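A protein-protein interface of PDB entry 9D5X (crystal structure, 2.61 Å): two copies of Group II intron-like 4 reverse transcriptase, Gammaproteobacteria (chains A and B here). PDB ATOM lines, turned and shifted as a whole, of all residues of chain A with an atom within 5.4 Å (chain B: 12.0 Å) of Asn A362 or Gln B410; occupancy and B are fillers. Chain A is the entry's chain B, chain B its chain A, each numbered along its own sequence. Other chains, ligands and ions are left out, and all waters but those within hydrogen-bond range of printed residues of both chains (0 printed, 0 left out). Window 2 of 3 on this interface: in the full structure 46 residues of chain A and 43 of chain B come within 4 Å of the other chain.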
ATOM      1  N   ARG A 131      29.617   0.889  23.626  1.00  0.00           N
ATOM      2  CA  ARG A 131      28.974   0.161  24.714  1.00  0.00           C
ATOM      3  C   ARG A 131      29.006  -1.342  24.467  1.00  0.00           C
ATOM      4  O   ARG A 131      29.221  -2.129  25.396  1.00  0.00           O
ATOM      5  CB  ARG A 131      27.535   0.648  24.885  1.00  0.00           C
ATOM      6  CG  ARG A 131      26.806   0.059  26.078  1.00  0.00           C
ATOM      7  CD  ARG A 131      25.406   0.635  26.187  1.00  0.00           C
ATOM      8  NE  ARG A 131      24.710   0.187  27.386  1.00  0.00           N
ATOM      9  CZ  ARG A 131      23.895  -0.858  27.431  1.00  0.00           C
ATOM     10  NH1 ARG A 131      23.662  -1.600  26.362  1.00  0.00           N
ATOM     11  NH2 ARG A 131      23.296  -1.162  28.578  1.00  0.00           N
ATOM     12  N   GLY A 298      27.268  -0.078  30.984  1.00  0.00           N
ATOM     13  CA  GLY A 298      25.862  -0.260  31.282  1.00  0.00           C
ATOM     14  C   GLY A 298      25.021   1.002  31.247  1.00  0.00           C
ATOM     15  O   GLY A 298      23.802   0.924  31.069  1.00  0.00           O
ATOM     16  N   LEU A 299      25.644   2.169  31.413  1.00  0.00           N
ATOM     17  CA  LEU A 299      24.923   3.430  31.533  1.00  0.00           C
ATOM     18  C   LEU A 299      25.395   4.416  30.475  1.00  0.00           C
ATOM     19  O   LEU A 299      26.594   4.698  30.374  1.00  0.00           O
ATOM     20  CB  LEU A 299      25.101   4.039  32.924  1.00  0.00           C
ATOM     21  CG  LEU A 299      24.270   5.299  33.169  1.00  0.00           C
ATOM     22  CD1 LEU A 299      22.792   4.946  33.204  1.00  0.00           C
ATOM     23  CD2 LEU A 299      24.690   6.003  34.451  1.00  0.00           C
ATOM     24  N   ILE A 300      24.449   4.947  29.705  1.00  0.00           N
ATOM     25  CA  ILE A 300      24.709   5.973  28.702  1.00  0.00           C
ATOM     26  C   ILE A 300      23.873   7.192  29.064  1.00  0.00           C
ATOM     27  O   ILE A 300      22.646   7.094  29.192  1.00  0.00           O
ATOM     28  CB  ILE A 300      24.375   5.489  27.282  1.00  0.00           C
ATOM     29  CG1 ILE A 300      24.981   4.107  27.027  1.00  0.00           C
ATOM     30  CG2 ILE A 300      24.866   6.492  26.247  1.00  0.00           C
ATOM     31  CD1 ILE A 300      26.484   4.060  27.138  1.00  0.00           C
ATOM     32  N   GLN A 301      24.531   8.334  29.226  1.00  0.00           N
ATOM     33  CA  GLN A 301      23.866   9.566  29.622  1.00  0.00           C
ATOM     34  C   GLN A 301      24.677  10.736  29.095  1.00  0.00           C
ATOM     35  O   GLN A 301      25.862  10.579  28.774  1.00  0.00           O
ATOM     36  CB  GLN A 301      23.724   9.656  31.147  1.00  0.00           C
ATOM     37  CG  GLN A 301      25.051   9.631  31.887  1.00  0.00           C
ATOM     38  CD  GLN A 301      24.880   9.601  33.391  1.00  0.00           C
ATOM     39  OE1 GLN A 301      23.797   9.876  33.911  1.00  0.00           O
ATOM     40  NE2 GLN A 301      25.950   9.258  34.102  1.00  0.00           N
ATOM     41  N   PHE A 358      19.297  13.242  22.726  1.00  0.00           N
ATOM     42  CA  PHE A 358      19.846  12.225  23.614  1.00  0.00           C
ATOM     43  C   PHE A 358      18.844  11.105  23.879  1.00  0.00           C
ATOM     44  O   PHE A 358      18.850  10.504  24.954  1.00  0.00           O
ATOM     45  CB  PHE A 358      20.311  12.848  24.930  1.00  0.00           C
ATOM     46  CG  PHE A 358      21.431  13.837  24.767  1.00  0.00           C
ATOM     47  CD1 PHE A 358      22.740  13.406  24.615  1.00  0.00           C
ATOM     48  CD2 PHE A 358      21.177  15.198  24.769  1.00  0.00           C
ATOM     49  CE1 PHE A 358      23.772  14.315  24.465  1.00  0.00           C
ATOM     50  CE2 PHE A 358      22.204  16.110  24.618  1.00  0.00           C
ATOM     51  CZ  PHE A 358      23.504  15.667  24.465  1.00  0.00           C
ATOM     52  N   THR A 359      17.984  10.809  22.900  1.00  0.00           N
ATOM     53  CA  THR A 359      17.025   9.722  23.063  1.00  0.00           C
ATOM     54  C   THR A 359      17.690   8.353  23.044  1.00  0.00           C
ATOM     55  O   THR A 359      17.064   7.369  23.454  1.00  0.00           O
ATOM     56  CB  THR A 359      15.952   9.784  21.975  1.00  0.00           C
ATOM     57  OG1 THR A 359      16.575   9.893  20.689  1.00  0.00           O
ATOM     58  CG2 THR A 359      15.032  10.976  22.198  1.00  0.00           C
ATOM     59  N   PHE A 360      18.935   8.260  22.573  1.00  0.00           N
ATOM     60  CA  PHE A 360      19.664   7.000  22.614  1.00  0.00           C
ATOM     61  C   PHE A 360      20.259   6.711  23.985  1.00  0.00           C
ATOM     62  O   PHE A 360      20.819   5.628  24.184  1.00  0.00           O
ATOM     63  CB  PHE A 360      20.769   6.988  21.550  1.00  0.00           C
ATOM     64  CG  PHE A 360      21.811   8.057  21.734  1.00  0.00           C
ATOM     65  CD1 PHE A 360      22.939   7.823  22.506  1.00  0.00           C
ATOM     66  CD2 PHE A 360      21.672   9.291  21.118  1.00  0.00           C
ATOM     67  CE1 PHE A 360      23.900   8.803  22.671  1.00  0.00           C
ATOM     68  CE2 PHE A 360      22.632  10.274  21.279  1.00  0.00           C
ATOM     69  CZ  PHE A 360      23.748  10.028  22.057  1.00  0.00           C
ATOM     70  N   CYS A 361      20.151   7.641  24.926  1.00  0.00           N
ATOM     71  CA  CYS A 361      20.669   7.451  26.271  1.00  0.00           C
ATOM     72  C   CYS A 361      19.648   6.736  27.146  1.00  0.00           C
ATOM     73  O   CYS A 361      18.436   6.883  26.970  1.00  0.00           O
ATOM     74  CB  CYS A 361      21.038   8.796  26.901  1.00  0.00           C
ATOM     75  SG  CYS A 361      22.444   9.625  26.126  1.00  0.00           S
ATOM     76  N   ASN A 362      20.155   5.957  28.101  1.00  0.00           N
ATOM     77  CA  ASN A 362      19.316   5.242  29.051  1.00  0.00           C
ATOM     78  C   ASN A 362      19.460   5.752  30.476  1.00  0.00           C
ATOM     79  O   ASN A 362      18.865   5.170  31.389  1.00  0.00           O
ATOM     80  CB  ASN A 362      19.627   3.741  29.007  1.00  0.00           C
ATOM     81  CG  ASN A 362      21.105   3.444  29.170  1.00  0.00           C
ATOM     82  OD1 ASN A 362      21.772   3.998  30.043  1.00  0.00           O
ATOM     83  ND2 ASN A 362      21.627   2.569  28.321  1.00  0.00           N
ATOM     84  N   GLY A 363      20.233   6.812  30.697  1.00  0.00           N
ATOM     85  CA  GLY A 363      20.360   7.377  32.024  1.00  0.00           C
ATOM     86  C   GLY A 363      19.135   8.169  32.432  1.00  0.00           C
ATOM     87  O   GLY A 363      18.950   9.308  31.995  1.00  0.00           O
ATOM     88  N   SER A 364      18.291   7.572  33.275  1.00  0.00           N
ATOM     89  CA  SER A 364      17.067   8.222  33.730  1.00  0.00           C
ATOM     90  C   SER A 364      17.282   9.127  34.932  1.00  0.00           C
ATOM     91  O   SER A 364      16.518  10.080  35.123  1.00  0.00           O
ATOM     92  CB  SER A 364      16.010   7.169  34.071  1.00  0.00           C
ATOM     93  OG  SER A 364      16.432   6.351  35.148  1.00  0.00           O
ATOM     94  N   MET A 367      18.227  12.716  33.827  1.00  0.00           N
ATOM     95  CA  MET A 367      17.080  13.381  33.216  1.00  0.00           C
ATOM     96  C   MET A 367      16.091  13.848  34.276  1.00  0.00           C
ATOM     97  O   MET A 367      15.566  14.965  34.193  1.00  0.00           O
ATOM     98  CB  MET A 367      16.398  12.447  32.218  1.00  0.00           C
ATOM     99  CG  MET A 367      17.253  12.108  31.008  1.00  0.00           C
ATOM    100  SD  MET A 367      17.816  13.576  30.128  1.00  0.00           S
ATOM    101  CE  MET A 367      18.867  12.842  28.877  1.00  0.00           C
ATOM    102  N   GLN B 332      -1.661  12.007  31.114  1.00  0.00           N
ATOM    103  CA  GLN B 332      -0.255  12.217  30.796  1.00  0.00           C
ATOM    104  C   GLN B 332       0.022  12.238  29.297  1.00  0.00           C
ATOM    105  O   GLN B 332       1.186  12.318  28.892  1.00  0.00           O
ATOM    106  CB  GLN B 332       0.600  11.141  31.470  1.00  0.00           C
ATOM    107  CG  GLN B 332       0.552  11.181  32.995  1.00  0.00           C
ATOM    108  CD  GLN B 332       1.417  10.112  33.634  1.00  0.00           C
ATOM    109  OE1 GLN B 332       1.938   9.232  32.952  1.00  0.00           O
ATOM    110  NE2 GLN B 332       1.574  10.184  34.953  1.00  0.00           N
ATOM    111  N   ARG B 398       3.943  20.771  35.366  1.00  0.00           N
ATOM    112  CA  ARG B 398       4.692  20.793  34.114  1.00  0.00           C
ATOM    113  C   ARG B 398       3.776  20.554  32.920  1.00  0.00           C
ATOM    114  O   ARG B 398       3.853  21.268  31.915  1.00  0.00           O
ATOM    115  CB  ARG B 398       5.811  19.750  34.158  1.00  0.00           C
ATOM    116  CG  ARG B 398       6.930  20.098  35.124  1.00  0.00           C
ATOM    117  CD  ARG B 398       7.828  21.181  34.558  1.00  0.00           C
ATOM    118  NE  ARG B 398       8.684  20.658  33.502  1.00  0.00           N
ATOM    119  CZ  ARG B 398       9.853  20.068  33.713  1.00  0.00           C
ATOM    120  NH1 ARG B 398      10.340  19.922  34.934  1.00  0.00           N
ATOM    121  NH2 ARG B 398      10.548  19.613  32.676  1.00  0.00           N
ATOM    122  N   ARG B 404       7.568  20.606  28.810  1.00  0.00           N
ATOM    123  CA  ARG B 404       7.731  19.164  28.682  1.00  0.00           C
ATOM    124  C   ARG B 404       8.697  18.612  29.726  1.00  0.00           C
ATOM    125  O   ARG B 404       9.545  19.324  30.275  1.00  0.00           O
ATOM    126  CB  ARG B 404       8.241  18.812  27.287  1.00  0.00           C
ATOM    127  CG  ARG B 404       7.276  18.017  26.430  1.00  0.00           C
ATOM    128  CD  ARG B 404       7.855  17.817  25.041  1.00  0.00           C
ATOM    129  NE  ARG B 404       8.028  19.085  24.344  1.00  0.00           N
ATOM    130  CZ  ARG B 404       7.171  19.571  23.457  1.00  0.00           C
ATOM    131  NH1 ARG B 404       6.082  18.905  23.113  1.00  0.00           N
ATOM    132  NH2 ARG B 404       7.413  20.755  22.901  1.00  0.00           N
ATOM    133  N   LEU B 405       8.562  17.315  29.987  1.00  0.00           N
ATOM    134  CA  LEU B 405       9.451  16.588  30.880  1.00  0.00           C
ATOM    135  C   LEU B 405      10.529  15.895  30.059  1.00  0.00           C
ATOM    136  O   LEU B 405      10.226  15.257  29.044  1.00  0.00           O
ATOM    137  CB  LEU B 405       8.676  15.562  31.708  1.00  0.00           C
ATOM    138  CG  LEU B 405       7.710  16.114  32.755  1.00  0.00           C
ATOM    139  CD1 LEU B 405       6.902  14.993  33.386  1.00  0.00           C
ATOM    140  CD2 LEU B 405       8.475  16.883  33.817  1.00  0.00           C
ATOM    141  N   LEU B 406      11.785  16.026  30.496  1.00  0.00           N
ATOM    142  CA  LEU B 406      12.879  15.352  29.810  1.00  0.00           C
ATOM    143  C   LEU B 406      12.765  13.837  29.919  1.00  0.00           C
ATOM    144  O   LEU B 406      13.180  13.119  29.003  1.00  0.00           O
ATOM    145  CB  LEU B 406      14.221  15.821  30.374  1.00  0.00           C
ATOM    146  CG  LEU B 406      14.717  17.193  29.921  1.00  0.00           C
ATOM    147  CD1 LEU B 406      15.853  17.669  30.807  1.00  0.00           C
ATOM    148  CD2 LEU B 406      15.166  17.140  28.470  1.00  0.00           C
ATOM    149  N   ILE B 407      12.205  13.334  31.022  1.00  0.00           N
ATOM    150  CA  ILE B 407      12.110  11.890  31.203  1.00  0.00           C
ATOM    151  C   ILE B 407      11.066  11.295  30.266  1.00  0.00           C
ATOM    152  O   ILE B 407      11.174  10.129  29.868  1.00  0.00           O
ATOM    153  CB  ILE B 407      11.818  11.558  32.680  1.00  0.00           C
ATOM    154  CG1 ILE B 407      11.997  10.060  32.943  1.00  0.00           C
ATOM    155  CG2 ILE B 407      10.423  12.022  33.081  1.00  0.00           C
ATOM    156  CD1 ILE B 407      13.423   9.577  32.773  1.00  0.00           C
ATOM    157  N   ASP B 408      10.053  12.076  29.882  1.00  0.00           N
ATOM    158  CA  ASP B 408       9.049  11.583  28.945  1.00  0.00           C
ATOM    159  C   ASP B 408       9.579  11.528  27.519  1.00  0.00           C
ATOM    160  O   ASP B 408       9.134  10.687  26.730  1.00  0.00           O
ATOM    161  CB  ASP B 408       7.793  12.454  29.007  1.00  0.00           C
ATOM    162  CG  ASP B 408       7.054  12.323  30.326  1.00  0.00           C
ATOM    163  OD1 ASP B 408       7.226  11.291  31.008  1.00  0.00           O
ATOM    164  OD2 ASP B 408       6.297  13.252  30.676  1.00  0.00           O
ATOM    165  N   ILE B 409      10.517  12.410  27.171  1.00  0.00           N
ATOM    166  CA  ILE B 409      11.125  12.361  25.845  1.00  0.00           C
ATOM    167  C   ILE B 409      12.005  11.125  25.712  1.00  0.00           C
ATOM    168  O   ILE B 409      11.981  10.433  24.685  1.00  0.00           O
ATOM    169  CB  ILE B 409      11.923  13.648  25.572  1.00  0.00           C
ATOM    170  CG1 ILE B 409      11.103  14.886  25.934  1.00  0.00           C
ATOM    171  CG2 ILE B 409      12.358  13.705  24.115  1.00  0.00           C
ATOM    172  CD1 ILE B 409      11.897  16.176  25.863  1.00  0.00           C
ATOM    173  N   GLN B 410      12.793  10.829  26.748  1.00  0.00           N
ATOM    174  CA  GLN B 410      13.710   9.694  26.702  1.00  0.00           C
ATOM    175  C   GLN B 410      12.966   8.366  26.677  1.00  0.00           C
ATOM    176  O   GLN B 410      13.428   7.412  26.042  1.00  0.00           O
ATOM    177  CB  GLN B 410      14.658   9.749  27.898  1.00  0.00           C
ATOM    178  CG  GLN B 410      15.876   8.852  27.784  1.00  0.00           C
ATOM    179  CD  GLN B 410      16.742   8.902  29.027  1.00  0.00           C
ATOM    180  OE1 GLN B 410      16.256   8.717  30.143  1.00  0.00           O
ATOM    181  NE2 GLN B 410      18.031   9.157  28.842  1.00  0.00           N
ATOM    182  N   ASN B 411      11.817   8.282  27.353  1.00  0.00           N
ATOM    183  CA  ASN B 411      11.048   7.041  27.351  1.00  0.00           C
ATOM    184  C   ASN B 411      10.520   6.712  25.963  1.00  0.00           C
ATOM    185  O   ASN B 411      10.326   5.534  25.638  1.00  0.00           O
ATOM    186  CB  ASN B 411       9.889   7.131  28.346  1.00  0.00           C
ATOM    187  CG  ASN B 411      10.361   7.201  29.786  1.00  0.00           C
ATOM    188  OD1 ASN B 411      11.502   6.858  30.097  1.00  0.00           O
ATOM    189  ND2 ASN B 411       9.480   7.643  30.676  1.00  0.00           N
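The backbone carbonyl oxygen of Cys A361 sits at hydrogen-bond distance from the side-chain amide nitrogen of Gln B410, 3.0 Å away.
The side-chain amide nitrogen (NE2) of Gln B410 lies within hydrogen-bond range of the backbone carbonyl oxygen (O) of Gly A363 (3.3 Å).
Thr A359 touches Ile B409 (CG2 to O, 3.97 Å).
Asn A362 touches Gln B410 (N to NE2, 3.9 Å).
Ser A364 touches Ile B407.
CA of Ser A364 touches OE1 of Gln B410, 3.7 Å away.
OE1 of Gln B410 touches CG of Met A367, at 3.6 Å.
Of the 13 printed residues of chain A, 6 touch a printed residue of chain B.
Printed residues of chain A that touch a printed residue of chain B: Thr A359, Cys A361, Asn A362, Gly A363, Ser A364 and Met A367.
Hydrophobic or aromatic side chains of chain A within 4 Å of the printed part of chain B: Met A367.
Hydrophobic or aromatic side chains of chain B that line the printed part of chain A: Ile B407.
Among the printed residues, no Asp or Glu carboxylate lies within 4 Å of a Lys or Arg side-chain nitrogen of the other chain.
No position is printed for both chains.
Of the 7 pairs that touch across the chains among the printed residues, none has its exchanged pair printed and touching as well.
No residue of chain B comes within 4 Å of Gly A298.
No residue of chain B comes within 4 Å of Leu A299.
No residue of chain B comes within 4 Å of Gln A301.
Thr A359 touches one residue of chain B.
Asn A362 touches one residue of chain B.
Of chain B, only Ile B407 and Gln B410 come within 4 Å of Ser A364.
Met A367 touches one residue of chain B.
Leu B405 touches none of the printed residues of chain A.
Leu B406 touches none of the printed residues of chain A.
Of the printed residues of chain A, Ile B407 touches Ser A364.
Of the printed residues of chain A, Ile B409 touches Thr A359.
The nearest residue of chain B that does not touch Asn A362 is Ile B407 (7.1 Å).
The nearest residue of chain A that does not touch Gln B410 is Phe A358 (4.2 Å).
The nearest printed residue of chain A that does not touch Ile B407 is Met A367 (4.2 Å).
The side-chain amide nitrogen (ND2) of Asn B411 lies close to the backbone carbonyl oxygen (O) of Ile B407.
The backbone NH of Ile A300 lies within hydrogen-bond range of the side-chain amide oxygen of Asn A362 (2.9 Å).
N of Gly A363 lies within hydrogen-bond range of O of Ile A300, at 2.9 Å.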
